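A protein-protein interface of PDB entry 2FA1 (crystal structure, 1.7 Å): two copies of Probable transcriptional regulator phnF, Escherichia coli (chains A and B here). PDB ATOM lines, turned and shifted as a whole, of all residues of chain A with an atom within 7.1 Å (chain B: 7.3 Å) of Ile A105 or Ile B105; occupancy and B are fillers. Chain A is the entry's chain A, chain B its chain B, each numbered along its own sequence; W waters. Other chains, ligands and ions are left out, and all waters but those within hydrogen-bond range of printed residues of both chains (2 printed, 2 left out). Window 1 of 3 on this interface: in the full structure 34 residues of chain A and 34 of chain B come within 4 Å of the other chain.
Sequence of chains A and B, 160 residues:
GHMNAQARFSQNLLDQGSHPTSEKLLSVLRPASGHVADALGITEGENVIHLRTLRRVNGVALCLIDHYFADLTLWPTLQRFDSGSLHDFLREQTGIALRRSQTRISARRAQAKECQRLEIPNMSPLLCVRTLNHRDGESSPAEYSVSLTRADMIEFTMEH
OE2 of Glu A155 lies within salt-bridge range of NH2 of Arg B130 (2.9 Å). The side-chain hydroxyl (OG) of Ser B106 sits at hydrogen-bond distance from the side-chain amide nitrogen (NE2) of Gln A6, at 2.6 Å. The backbone carbonyl oxygen of Thr A103 sits at hydrogen-bond distance from the backbone NH of Met B158 (2.9 Å). The guanidinium group (NH2) of Arg A130 lies within salt-bridge range of the side-chain carboxylate (OE2) of Glu B155 (2.7 Å). The backbone NH (N) of Met A158 sits at hydrogen-bond distance from the backbone carbonyl oxygen (O) of Thr B103, 2.9 Å away. The backbone NH (N) of Ile A105 lies within hydrogen-bond range of the backbone carbonyl oxygen (O) of Phe B156 (2.9 Å). SD of Met A158 lies close to SD of Met B158, at 3.6 Å. The side-chain carboxylate (OE1) of Glu B155 lies within salt-bridge range of the guanidinium group (NH1) of Arg A104 (2.9 Å). N of Ile B105 lies within hydrogen-bond range of O of Phe A156, at 2.7 Å. OE1 of Glu A155 is in salt-bridge range of NH1 of Arg B104, 2.8 Å away.
Water W1 bridges the backbone carbonyl oxygen (O) of Ile B154 (2.6 Å) and the backbone NH (N) of Ala A107 (2.9 Å). Water W2 lies within hydrogen-bond range of N of Ala B107 and O of Ile A154.
The guanidinium group of Arg B100 sits close to the side-chain hydroxyl of Thr B103. O of Arg A130 lies within hydrogen-bond range of N of Arg A104 (2.8 Å). OE1 of Glu A155 is in hydrogen-bond range of N of Gln A6. The backbone carbonyl oxygen (O) of Glu A155 lies within hydrogen-bond range of the backbone NH (N) of Gln A11 (2.9 Å). The backbone carbonyl oxygen (O) of Ser B106 sits at hydrogen-bond distance from the backbone NH (N) of Cys B128 (2.8 Å). The backbone carbonyl oxygen (O) of Gln A11 is in hydrogen-bond range of the backbone NH (N) of Thr A157 (2.9 Å).
Printed residues of chain A that touch a printed residue of chain B: Gln A6, Leu A13, Thr A103, Arg A104, Ile A105, Ser A106, Ala A107, Leu A127, Arg A130, Glu A155, Phe A156, Thr A157 and Met A158. Hydrophobic or aromatic side chains of chain B that line the printed part of chain A: Leu B13, Ile B105, Ala B107, Leu B127, Phe B156 and Met B158. Among the printed residues, 30 pairs touch across the chains. Among the printed residues, Asp or Glu carboxylates within 4 Å of a Lys or Arg side-chain nitrogen of the other chain: Arg A104 with Glu B155, Arg A130 with Glu B155, Glu A155 with Arg B104 and Glu A155 with Arg B130.
Ile B105 touches three residues of chain A. Of the printed residues of chain A, Arg B130 touches Gln A6 (3.4 Å) and Glu A155 (2.9 Å). Of the printed residues of chain B, Ala A107 touches Ala B107 and Leu B127. Thr B131 touches none of the printed residues of chain A. The nearest residue of chain A that does not touch Ile B105 is Leu A127 (4.1 Å). The nearest printed residue of chain A that does not touch Cys B128 is Glu A155 (5.6 Å).
Thr A103 touches Thr B157, and with the chains exchanged Thr A157 touches Thr B103. Ile B105 touches its own counterpart, Ile A105. Ser A106 touches Glu B155, and with the chains exchanged Glu A155 touches Ser B106. Arg A130 touches Glu B155, and with the chains exchanged Glu A155 touches Arg B130.
Among the printed residues, pairs that only touch across the chains: Arg A104 with Phe B156, Phe A156 with Arg B104, Thr A157 with Arg B104, Thr A103 with Thr B157, Thr A157 with Thr B103, Gln A6 with Arg B130, Ile A105 with Glu B155, Arg A104 with Thr B157, Glu A155 with Ile B105, Leu A13 with Met B158, Glu A155 with Ser B106, Ile A105 with Ile B105, Met A158 with Leu B13, Leu A127 with Leu B127, Ala A107 with Ala B107, Leu A127 with Ala B107, Gln A6 with Cys B128, Ser A106 with Glu B155, Thr A103 with Phe B156 and Ala A107 with Leu B127.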
ATOM      1  N   GLN A   6     -30.983  24.189   1.649  1.00  0.00           N
ATOM      2  CA  GLN A   6     -29.624  24.167   2.194  1.00  0.00           C
ATOM      3  C   GLN A   6     -29.025  25.569   2.271  1.00  0.00           C
ATOM      4  O   GLN A   6     -27.850  25.737   2.635  1.00  0.00           O
ATOM      5  CB  GLN A   6     -28.658  23.350   1.295  1.00  0.00           C
ATOM      6  CG  GLN A   6     -28.936  21.869   1.228  1.00  0.00           C
ATOM      7  CD  GLN A   6     -27.669  21.028   1.168  1.00  0.00           C
ATOM      8  OE1 GLN A   6     -27.632  19.909   1.714  1.00  0.00           O
ATOM      9  NE2 GLN A   6     -26.620  21.549   0.483  1.00  0.00           N
ATOM     10  N   GLN A  11     -33.445  30.118  -5.722  1.00  0.00           N
ATOM     11  CA  GLN A  11     -33.715  30.732  -7.037  1.00  0.00           C
ATOM     12  C   GLN A  11     -34.016  29.624  -8.046  1.00  0.00           C
ATOM     13  O   GLN A  11     -33.301  28.641  -8.124  1.00  0.00           O
ATOM     14  CB  GLN A  11     -32.559  31.643  -7.571  1.00  0.00           C
ATOM     15  CG  GLN A  11     -32.430  33.129  -6.960  1.00  0.00           C
ATOM     16  CD  GLN A  11     -31.127  33.921  -7.362  1.00  0.00           C
ATOM     17  OE1 GLN A  11     -31.024  35.149  -7.134  1.00  0.00           O
ATOM     18  NE2 GLN A  11     -30.154  33.226  -7.982  1.00  0.00           N
ATOM     19  N   LEU A  13     -33.810  27.678 -11.248  1.00  0.00           N
ATOM     20  CA  LEU A  13     -32.719  27.529 -12.211  1.00  0.00           C
ATOM     21  C   LEU A  13     -33.245  27.903 -13.585  1.00  0.00           C
ATOM     22  O   LEU A  13     -32.512  28.423 -14.404  1.00  0.00           O
ATOM     23  CB  LEU A  13     -32.167  26.074 -12.171  1.00  0.00           C
ATOM     24  CG  LEU A  13     -30.978  25.777 -13.090  1.00  0.00           C
ATOM     25  CD1 LEU A  13     -29.746  26.565 -12.616  1.00  0.00           C
ATOM     26  CD2 LEU A  13     -30.686  24.323 -13.104  1.00  0.00           C
ATOM     27  N   THR A 103     -27.466  25.015 -20.503  1.00  0.00           N
ATOM     28  CA  THR A 103     -27.108  25.529 -19.159  1.00  0.00           C
ATOM     29  C   THR A 103     -25.860  24.741 -18.751  1.00  0.00           C
ATOM     30  O   THR A 103     -25.789  23.507 -19.035  1.00  0.00           O
ATOM     31  CB  THR A 103     -28.222  25.312 -18.120  1.00  0.00           C
ATOM     32  OG1 THR A 103     -29.465  25.901 -18.548  1.00  0.00           O
ATOM     33  CG2 THR A 103     -27.834  25.945 -16.740  1.00  0.00           C
ATOM     34  N   ARG A 104     -24.870  25.435 -18.141  1.00  0.00           N
ATOM     35  CA  ARG A 104     -23.727  24.722 -17.524  1.00  0.00           C
ATOM     36  C   ARG A 104     -23.656  25.210 -16.072  1.00  0.00           C
ATOM     37  O   ARG A 104     -23.645  26.421 -15.873  1.00  0.00           O
ATOM     38  CB  ARG A 104     -22.457  24.977 -18.210  1.00  0.00           C
ATOM     39  CG  ARG A 104     -22.385  24.222 -19.577  1.00  0.00           C
ATOM     40  CD  ARG A 104     -20.897  24.283 -20.090  1.00  0.00           C
ATOM     41  NE  ARG A 104     -20.728  23.216 -21.047  1.00  0.00           N
ATOM     42  CZ  ARG A 104     -20.032  22.082 -20.854  1.00  0.00           C
ATOM     43  NH1 ARG A 104     -19.350  21.815 -19.732  1.00  0.00           N
ATOM     44  NH2 ARG A 104     -20.022  21.208 -21.846  1.00  0.00           N
ATOM     45  N   ILE A 105     -23.563  24.300 -15.088  1.00  0.00           N
ATOM     46  CA  ILE A 105     -23.495  24.695 -13.688  1.00  0.00           C
ATOM     47  C   ILE A 105     -22.175  24.176 -13.103  1.00  0.00           C
ATOM     48  O   ILE A 105     -21.836  23.003 -13.249  1.00  0.00           O
ATOM     49  CB  ILE A 105     -24.652  24.077 -12.929  1.00  0.00           C
ATOM     50  CG1 ILE A 105     -25.925  24.576 -13.611  1.00  0.00           C
ATOM     51  CG2 ILE A 105     -24.664  24.597 -11.426  1.00  0.00           C
ATOM     52  CD1 ILE A 105     -27.035  23.788 -13.157  1.00  0.00           C
ATOM     53  N   SER A 106     -21.376  25.098 -12.562  1.00  0.00           N
ATOM     54  CA  SER A 106     -20.171  24.643 -11.859  1.00  0.00           C
ATOM     55  C   SER A 106     -20.047  25.308 -10.496  1.00  0.00           C
ATOM     56  O   SER A 106     -20.780  26.212 -10.175  1.00  0.00           O
ATOM     57  CB  SER A 106     -18.964  25.038 -12.686  1.00  0.00           C
ATOM     58  OG  SER A 106     -18.905  26.437 -12.915  1.00  0.00           O
ATOM     59  N   ALA A 107     -19.000  24.918  -9.761  1.00  0.00           N
ATOM     60  CA  ALA A 107     -18.768  25.610  -8.446  1.00  0.00           C
ATOM     61  C   ALA A 107     -17.297  25.831  -8.365  1.00  0.00           C
ATOM     62  O   ALA A 107     -16.487  24.984  -8.758  1.00  0.00           O
ATOM     63  CB  ALA A 107     -19.248  24.844  -7.247  1.00  0.00           C
ATOM     64  N   LEU A 127     -21.434  29.491  -6.860  1.00  0.00           N
ATOM     65  CA  LEU A 127     -22.079  28.676  -7.904  1.00  0.00           C
ATOM     66  C   LEU A 127     -21.979  29.511  -9.159  1.00  0.00           C
ATOM     67  O   LEU A 127     -22.252  30.759  -9.129  1.00  0.00           O
ATOM     68  CB  LEU A 127     -23.556  28.441  -7.601  1.00  0.00           C
ATOM     69  CG  LEU A 127     -23.843  27.269  -6.656  1.00  0.00           C
ATOM     70  CD1 LEU A 127     -25.211  27.338  -5.846  1.00  0.00           C
ATOM     71  CD2 LEU A 127     -23.665  25.973  -7.440  1.00  0.00           C
ATOM     72  N   CYS A 128     -21.561  28.895 -10.271  1.00  0.00           N
ATOM     73  CA  CYS A 128     -21.456  29.616 -11.505  1.00  0.00           C
ATOM     74  C   CYS A 128     -22.435  28.982 -12.502  1.00  0.00           C
ATOM     75  O   CYS A 128     -22.355  27.755 -12.729  1.00  0.00           O
ATOM     76  CB  CYS A 128     -20.060  29.546 -12.010  1.00  0.00           C
ATOM     77  SG  CYS A 128     -19.830  30.190 -13.740  1.00  0.00           S
ATOM     78  N   VAL A 129     -23.392  29.775 -13.026  1.00  0.00           N
ATOM     79  CA  VAL A 129     -24.437  29.210 -13.915  1.00  0.00           C
ATOM     80  C   VAL A 129     -24.277  29.960 -15.237  1.00  0.00           C
ATOM     81  O   VAL A 129     -24.356  31.223 -15.287  1.00  0.00           O
ATOM     82  CB  VAL A 129     -25.881  29.340 -13.391  1.00  0.00           C
ATOM     83  CG1 VAL A 129     -26.834  28.771 -14.401  1.00  0.00           C
ATOM     84  CG2 VAL A 129     -26.044  28.576 -12.079  1.00  0.00           C
ATOM     85  N   ARG A 130     -24.083  29.213 -16.321  1.00  0.00           N
ATOM     86  CA  ARG A 130     -23.771  29.899 -17.614  1.00  0.00           C
ATOM     87  C   ARG A 130     -24.824  29.390 -18.562  1.00  0.00           C
ATOM     88  O   ARG A 130     -25.175  28.169 -18.576  1.00  0.00           O
ATOM     89  CB  ARG A 130     -22.398  29.535 -18.155  1.00  0.00           C
ATOM     90  CG  ARG A 130     -21.208  29.989 -17.235  1.00  0.00           C
ATOM     91  CD  ARG A 130     -19.897  29.874 -17.865  1.00  0.00           C
ATOM     92  NE  ARG A 130     -19.491  28.489 -17.912  1.00  0.00           N
ATOM     93  CZ  ARG A 130     -18.975  27.863 -18.978  1.00  0.00           C
ATOM     94  NH1 ARG A 130     -18.756  28.482 -20.119  1.00  0.00           N
ATOM     95  NH2 ARG A 130     -18.608  26.585 -18.853  1.00  0.00           N
ATOM     96  N   ILE A 154     -27.434  31.115  -1.585  1.00  0.00           N
ATOM     97  CA  ILE A 154     -28.460  30.741  -2.601  1.00  0.00           C
ATOM     98  C   ILE A 154     -28.311  29.308  -3.067  1.00  0.00           C
ATOM     99  O   ILE A 154     -27.161  28.894  -3.317  1.00  0.00           O
ATOM    100  CB  ILE A 154     -28.392  31.695  -3.820  1.00  0.00           C
ATOM    101  CG1 ILE A 154     -28.972  33.100  -3.546  1.00  0.00           C
ATOM    102  CG2 ILE A 154     -29.230  31.125  -5.001  1.00  0.00           C
ATOM    103  CD1 ILE A 154     -28.538  34.154  -4.606  1.00  0.00           C
ATOM    104  N   GLU A 155     -29.453  28.568  -3.121  1.00  0.00           N
ATOM    105  CA  GLU A 155     -29.549  27.232  -3.726  1.00  0.00           C
ATOM    106  C   GLU A 155     -30.502  27.332  -4.929  1.00  0.00           C
ATOM    107  O   GLU A 155     -31.430  28.168  -4.949  1.00  0.00           O
ATOM    108  CB  GLU A 155     -30.035  26.247  -2.629  1.00  0.00           C
ATOM    109  CG  GLU A 155     -30.610  24.911  -3.150  1.00  0.00           C
ATOM    110  CD  GLU A 155     -30.871  23.922  -2.018  1.00  0.00           C
ATOM    111  OE1 GLU A 155     -31.723  24.255  -1.165  1.00  0.00           O
ATOM    112  OE2 GLU A 155     -30.269  22.800  -1.968  1.00  0.00           O
ATOM    113  N   PHE A 156     -30.251  26.546  -5.963  1.00  0.00           N
ATOM    114  CA  PHE A 156     -31.098  26.578  -7.155  1.00  0.00           C
ATOM    115  C   PHE A 156     -32.087  25.470  -7.103  1.00  0.00           C
ATOM    116  O   PHE A 156     -31.766  24.386  -6.646  1.00  0.00           O
ATOM    117  CB  PHE A 156     -30.283  26.445  -8.432  1.00  0.00           C
ATOM    118  CG  PHE A 156     -29.488  27.711  -8.773  1.00  0.00           C
ATOM    119  CD1 PHE A 156     -30.118  28.746  -9.430  1.00  0.00           C
ATOM    120  CD2 PHE A 156     -28.119  27.798  -8.473  1.00  0.00           C
ATOM    121  CE1 PHE A 156     -29.384  29.969  -9.704  1.00  0.00           C
ATOM    122  CE2 PHE A 156     -27.384  28.967  -8.743  1.00  0.00           C
ATOM    123  CZ  PHE A 156     -28.015  30.029  -9.381  1.00  0.00           C
ATOM    124  N   THR A 157     -33.292  25.738  -7.642  1.00  0.00           N
ATOM    125  CA  THR A 157     -34.307  24.675  -7.658  1.00  0.00           C
ATOM    126  C   THR A 157     -34.773  24.457  -9.096  1.00  0.00           C
ATOM    127  O   THR A 157     -34.704  25.369  -9.911  1.00  0.00           O
ATOM    128  CB  THR A 157     -35.553  25.052  -6.779  1.00  0.00           C
ATOM    129  OG1 THR A 157     -36.093  26.283  -7.255  1.00  0.00           O
ATOM    130  CG2 THR A 157     -35.117  25.225  -5.326  1.00  0.00           C
ATOM    131  N   MET A 158     -35.324  23.286  -9.389  1.00  0.00           N
ATOM    132  CA  MET A 158     -35.909  23.114 -10.722  1.00  0.00           C
ATOM    133  C   MET A 158     -37.083  22.160 -10.578  1.00  0.00           C
ATOM    134  O   MET A 158     -37.015  21.193  -9.804  1.00  0.00           O
ATOM    135  CB  MET A 158     -34.837  22.631 -11.721  1.00  0.00           C
ATOM    136  CG  MET A 158     -35.341  22.015 -13.001  1.00  0.00           C
ATOM    137  SD  MET A 158     -33.934  21.848 -14.083  1.00  0.00           S
ATOM    138  CE  MET A 158     -32.740  21.334 -12.857  1.00  0.00           C
ATOM    139  N   ALA B   7     -14.438  22.503 -16.482  1.00  0.00           N
ATOM    140  CA  ALA B   7     -13.968  21.450 -15.615  1.00  0.00           C
ATOM    141  C   ALA B   7     -13.523  20.293 -16.509  1.00  0.00           C
ATOM    142  O   ALA B   7     -13.855  20.255 -17.715  1.00  0.00           O
ATOM    143  CB  ALA B   7     -15.044  21.002 -14.687  1.00  0.00           C
ATOM    144  N   GLN B  11     -20.963  16.508 -17.183  1.00  0.00           N
ATOM    145  CA  GLN B  11     -21.954  15.507 -16.837  1.00  0.00           C
ATOM    146  C   GLN B  11     -23.373  16.040 -17.040  1.00  0.00           C
ATOM    147  O   GLN B  11     -23.736  17.071 -16.508  1.00  0.00           O
ATOM    148  CB  GLN B  11     -21.727  15.056 -15.405  1.00  0.00           C
ATOM    149  CG  GLN B  11     -22.805  14.128 -14.885  1.00  0.00           C
ATOM    150  CD  GLN B  11     -22.934  12.834 -15.696  1.00  0.00           C
ATOM    151  OE1 GLN B  11     -21.955  12.134 -15.935  1.00  0.00           O
ATOM    152  NE2 GLN B  11     -24.135  12.540 -16.159  1.00  0.00           N
ATOM    153  N   LEU B  13     -26.995  16.779 -16.270  1.00  0.00           N
ATOM    154  CA  LEU B  13     -27.612  16.850 -14.919  1.00  0.00           C
ATOM    155  C   LEU B  13     -28.641  15.753 -14.783  1.00  0.00           C
ATOM    156  O   LEU B  13     -28.708  15.052 -13.755  1.00  0.00           O
ATOM    157  CB  LEU B  13     -28.234  18.260 -14.784  1.00  0.00           C
ATOM    158  CG  LEU B  13     -28.742  18.708 -13.416  1.00  0.00           C
ATOM    159  CD1 LEU B  13     -27.701  18.524 -12.270  1.00  0.00           C
ATOM    160  CD2 LEU B  13     -29.228  20.126 -13.584  1.00  0.00           C
ATOM    161  N   ARG B 100     -37.873  12.288 -12.677  1.00  0.00           N
ATOM    162  CA  ARG B 100     -37.572  13.359 -11.772  1.00  0.00           C
ATOM    163  C   ARG B 100     -38.766  14.269 -11.542  1.00  0.00           C
ATOM    164  O   ARG B 100     -39.441  14.627 -12.509  1.00  0.00           O
ATOM    165  CB  ARG B 100     -36.410  14.142 -12.357  1.00  0.00           C
ATOM    166  CG  ARG B 100     -35.592  14.751 -11.349  1.00  0.00           C
ATOM    167  CD  ARG B 100     -34.440  15.410 -11.999  1.00  0.00           C
ATOM    168  NE  ARG B 100     -33.407  14.439 -12.348  1.00  0.00           N
ATOM    169  CZ  ARG B 100     -32.115  14.715 -12.289  1.00  0.00           C
ATOM    170  NH1 ARG B 100     -31.731  15.922 -11.863  1.00  0.00           N
ATOM    171  NH2 ARG B 100     -31.228  13.792 -12.634  1.00  0.00           N
ATOM    172  N   THR B 103     -35.546  19.128  -8.372  1.00  0.00           N
ATOM    173  CA  THR B 103     -34.037  19.013  -8.201  1.00  0.00           C
ATOM    174  C   THR B 103     -33.645  20.248  -7.415  1.00  0.00           C
ATOM    175  O   THR B 103     -34.225  21.316  -7.636  1.00  0.00           O
ATOM    176  CB  THR B 103     -33.277  19.088  -9.554  1.00  0.00           C
ATOM    177  OG1 THR B 103     -33.660  17.980 -10.411  1.00  0.00           O
ATOM    178  CG2 THR B 103     -31.817  18.929  -9.290  1.00  0.00           C
ATOM    179  N   ARG B 104     -32.717  20.097  -6.469  1.00  0.00           N
ATOM    180  CA  ARG B 104     -32.109  21.254  -5.749  1.00  0.00           C
ATOM    181  C   ARG B 104     -30.605  21.191  -5.967  1.00  0.00           C
ATOM    182  O   ARG B 104     -29.988  20.116  -5.728  1.00  0.00           O
ATOM    183  CB  ARG B 104     -32.414  21.293  -4.267  1.00  0.00           C
ATOM    184  CG  ARG B 104     -33.812  21.849  -3.961  1.00  0.00           C
ATOM    185  CD  ARG B 104     -34.011  22.139  -2.451  1.00  0.00           C
ATOM    186  NE  ARG B 104     -35.249  22.927  -2.359  1.00  0.00           N
ATOM    187  CZ  ARG B 104     -35.332  24.244  -2.172  1.00  0.00           C
ATOM    188  NH1 ARG B 104     -34.253  25.038  -2.008  1.00  0.00           N
ATOM    189  NH2 ARG B 104     -36.540  24.792  -2.143  1.00  0.00           N
ATOM    190  N   ILE B 105     -29.982  22.326  -6.285  1.00  0.00           N
ATOM    191  CA  ILE B 105     -28.520  22.326  -6.500  1.00  0.00           C
ATOM    192  C   ILE B 105     -27.840  23.391  -5.663  1.00  0.00           C
ATOM    193  O   ILE B 105     -28.245  24.556  -5.702  1.00  0.00           O
ATOM    194  CB  ILE B 105     -28.206  22.689  -7.981  1.00  0.00           C
ATOM    195  CG1 ILE B 105     -28.838  21.650  -8.926  1.00  0.00           C
ATOM    196  CG2 ILE B 105     -26.671  22.687  -8.244  1.00  0.00           C
ATOM    197  CD1 ILE B 105     -28.346  21.787 -10.333  1.00  0.00           C
ATOM    198  N   SER B 106     -26.807  22.981  -4.914  1.00  0.00           N
ATOM    199  CA  SER B 106     -26.165  23.877  -3.979  1.00  0.00           C
ATOM    200  C   SER B 106     -24.681  23.543  -4.002  1.00  0.00           C
ATOM    201  O   SER B 106     -24.267  22.574  -4.622  1.00  0.00           O
ATOM    202  CB  SER B 106     -26.775  23.643  -2.572  1.00  0.00           C
ATOM    203  OG  SER B 106     -26.398  22.393  -2.010  1.00  0.00           O
ATOM    204  N   ALA B 107     -23.865  24.425  -3.448  1.00  0.00           N
ATOM    205  CA  ALA B 107     -22.457  24.131  -3.364  1.00  0.00           C
ATOM    206  C   ALA B 107     -22.044  24.415  -1.920  1.00  0.00           C
ATOM    207  O   ALA B 107     -22.518  25.337  -1.287  1.00  0.00           O
ATOM    208  CB  ALA B 107     -21.688  24.929  -4.329  1.00  0.00           C
ATOM    209  N   LEU B 127     -20.328  20.099  -5.252  1.00  0.00           N
ATOM    210  CA  LEU B 127     -21.626  20.398  -5.795  1.00  0.00           C
ATOM    211  C   LEU B 127     -22.589  19.383  -5.243  1.00  0.00           C
ATOM    212  O   LEU B 127     -22.284  18.164  -5.330  1.00  0.00           O
ATOM    213  CB  LEU B 127     -21.564  20.248  -7.329  1.00  0.00           C
ATOM    214  CG  LEU B 127     -21.179  21.471  -8.110  1.00  0.00           C
ATOM    215  CD1 LEU B 127     -20.700  20.993  -9.545  1.00  0.00           C
ATOM    216  CD2 LEU B 127     -22.404  22.462  -8.141  1.00  0.00           C
ATOM    217  N   CYS B 128     -23.743  19.841  -4.704  1.00  0.00           N
ATOM    218  CA  CYS B 128     -24.655  18.876  -4.029  1.00  0.00           C
ATOM    219  C   CYS B 128     -25.939  18.952  -4.888  1.00  0.00           C
ATOM    220  O   CYS B 128     -26.525  20.062  -5.049  1.00  0.00           O
ATOM    221  CB  CYS B 128     -24.845  19.359  -2.611  1.00  0.00           C
ATOM    222  SG  CYS B 128     -26.216  18.443  -1.774  1.00  0.00           S
ATOM    223  N   VAL B 129     -26.409  17.827  -5.394  1.00  0.00           N
ATOM    224  CA  VAL B 129     -27.586  17.789  -6.241  1.00  0.00           C
ATOM    225  C   VAL B 129     -28.549  16.853  -5.522  1.00  0.00           C
ATOM    226  O   VAL B 129     -28.251  15.679  -5.292  1.00  0.00           O
ATOM    227  CB  VAL B 129     -27.277  17.306  -7.657  1.00  0.00           C
ATOM    228  CG1 VAL B 129     -28.639  17.169  -8.432  1.00  0.00           C
ATOM    229  CG2 VAL B 129     -26.276  18.192  -8.388  1.00  0.00           C
ATOM    230  N   ARG B 130     -29.708  17.375  -5.173  1.00  0.00           N
ATOM    231  CA  ARG B 130     -30.679  16.573  -4.420  1.00  0.00           C
ATOM    232  C   ARG B 130     -31.915  16.468  -5.289  1.00  0.00           C
ATOM    233  O   ARG B 130     -32.413  17.432  -5.817  1.00  0.00           O
ATOM    234  CB  ARG B 130     -30.940  17.225  -3.065  1.00  0.00           C
ATOM    235  CG  ARG B 130     -29.642  17.275  -2.244  1.00  0.00           C
ATOM    236  CD  ARG B 130     -29.933  17.739  -0.885  1.00  0.00           C
ATOM    237  NE  ARG B 130     -30.361  19.152  -0.902  1.00  0.00           N
ATOM    238  CZ  ARG B 130     -31.473  19.616  -0.297  1.00  0.00           C
ATOM    239  NH1 ARG B 130     -32.253  18.788   0.360  1.00  0.00           N
ATOM    240  NH2 ARG B 130     -31.788  20.927  -0.334  1.00  0.00           N
ATOM    241  N   THR B 131     -32.413  15.244  -5.470  1.00  0.00           N
ATOM    242  CA  THR B 131     -33.523  15.021  -6.416  1.00  0.00           C
ATOM    243  C   THR B 131     -34.567  14.102  -5.815  1.00  0.00           C
ATOM    244  O   THR B 131     -34.246  13.117  -5.156  1.00  0.00           O
ATOM    245  CB  THR B 131     -33.048  14.331  -7.739  1.00  0.00           C
ATOM    246  OG1 THR B 131     -32.463  13.064  -7.439  1.00  0.00           O
ATOM    247  CG2 THR B 131     -31.993  15.179  -8.554  1.00  0.00           C
ATOM    248  N   ILE B 154     -15.934  18.264 -12.061  1.00  0.00           N
ATOM    249  CA  ILE B 154     -17.137  18.078 -12.913  1.00  0.00           C
ATOM    250  C   ILE B 154     -17.941  19.394 -13.024  1.00  0.00           C
ATOM    251  O   ILE B 154     -18.044  20.162 -12.051  1.00  0.00           O
ATOM    252  CB  ILE B 154     -18.076  16.920 -12.383  1.00  0.00           C
ATOM    253  CG1 ILE B 154     -17.484  15.504 -12.688  1.00  0.00           C
ATOM    254  CG2 ILE B 154     -19.488  17.008 -12.982  1.00  0.00           C
ATOM    255  CD1 ILE B 154     -18.138  14.334 -11.833  1.00  0.00           C
ATOM    256  N   GLU B 155     -18.427  19.635 -14.236  1.00  0.00           N
ATOM    257  CA  GLU B 155     -19.436  20.725 -14.477  1.00  0.00           C
ATOM    258  C   GLU B 155     -20.706  20.019 -14.987  1.00  0.00           C
ATOM    259  O   GLU B 155     -20.605  19.102 -15.808  1.00  0.00           O
ATOM    260  CB  GLU B 155     -18.812  21.700 -15.477  1.00  0.00           C
ATOM    261  CG  GLU B 155     -19.694  22.867 -15.933  1.00  0.00           C
ATOM    262  CD  GLU B 155     -19.002  23.904 -16.835  1.00  0.00           C
ATOM    263  OE1 GLU B 155     -18.152  23.467 -17.658  1.00  0.00           O
ATOM    264  OE2 GLU B 155     -19.244  25.165 -16.617  1.00  0.00           O
ATOM    265  N   PHE B 156     -21.895  20.429 -14.528  1.00  0.00           N
ATOM    266  CA  PHE B 156     -23.131  19.843 -15.049  1.00  0.00           C
ATOM    267  C   PHE B 156     -23.640  20.565 -16.266  1.00  0.00           C
ATOM    268  O   PHE B 156     -23.435  21.760 -16.408  1.00  0.00           O
ATOM    269  CB  PHE B 156     -24.197  19.918 -13.959  1.00  0.00           C
ATOM    270  CG  PHE B 156     -23.887  19.009 -12.835  1.00  0.00           C
ATOM    271  CD1 PHE B 156     -23.841  17.621 -13.043  1.00  0.00           C
ATOM    272  CD2 PHE B 156     -23.728  19.508 -11.556  1.00  0.00           C
ATOM    273  CE1 PHE B 156     -23.581  16.736 -11.965  1.00  0.00           C
ATOM    274  CE2 PHE B 156     -23.466  18.620 -10.508  1.00  0.00           C
ATOM    275  CZ  PHE B 156     -23.396  17.239 -10.723  1.00  0.00           C
ATOM    276  N   THR B 157     -24.255  19.782 -17.169  1.00  0.00           N
ATOM    277  CA  THR B 157     -24.832  20.375 -18.371  1.00  0.00           C
ATOM    278  C   THR B 157     -26.315  20.022 -18.475  1.00  0.00           C
ATOM    279  O   THR B 157     -26.789  19.063 -17.905  1.00  0.00           O
ATOM    280  CB  THR B 157     -24.129  19.893 -19.628  1.00  0.00           C
ATOM    281  OG1 THR B 157     -24.321  18.452 -19.709  1.00  0.00           O
ATOM    282  CG2 THR B 157     -22.651  20.212 -19.577  1.00  0.00           C
ATOM    283  N   MET B 158     -27.049  20.884 -19.169  1.00  0.00           N
ATOM    284  CA  MET B 158     -28.461  20.582 -19.402  1.00  0.00           C
ATOM    285  C   MET B 158     -28.811  21.168 -20.748  1.00  0.00           C
ATOM    286  O   MET B 158     -28.466  22.306 -21.035  1.00  0.00           O
ATOM    287  CB  MET B 158     -29.303  21.133 -18.262  1.00  0.00           C
ATOM    288  CG  MET B 158     -30.848  20.938 -18.375  1.00  0.00           C
ATOM    289  SD  MET B 158     -31.728  21.277 -16.835  1.00  0.00           S
ATOM    290  CE  MET B 158     -30.691  22.450 -16.101  1.00  0.00           C
HETATM  291  O   HOH W   1     -17.752  22.526 -10.910  1.00  0.00           O
HETATM  292  O   HOH W   2     -25.412  26.694  -2.475  1.00  0.00           O
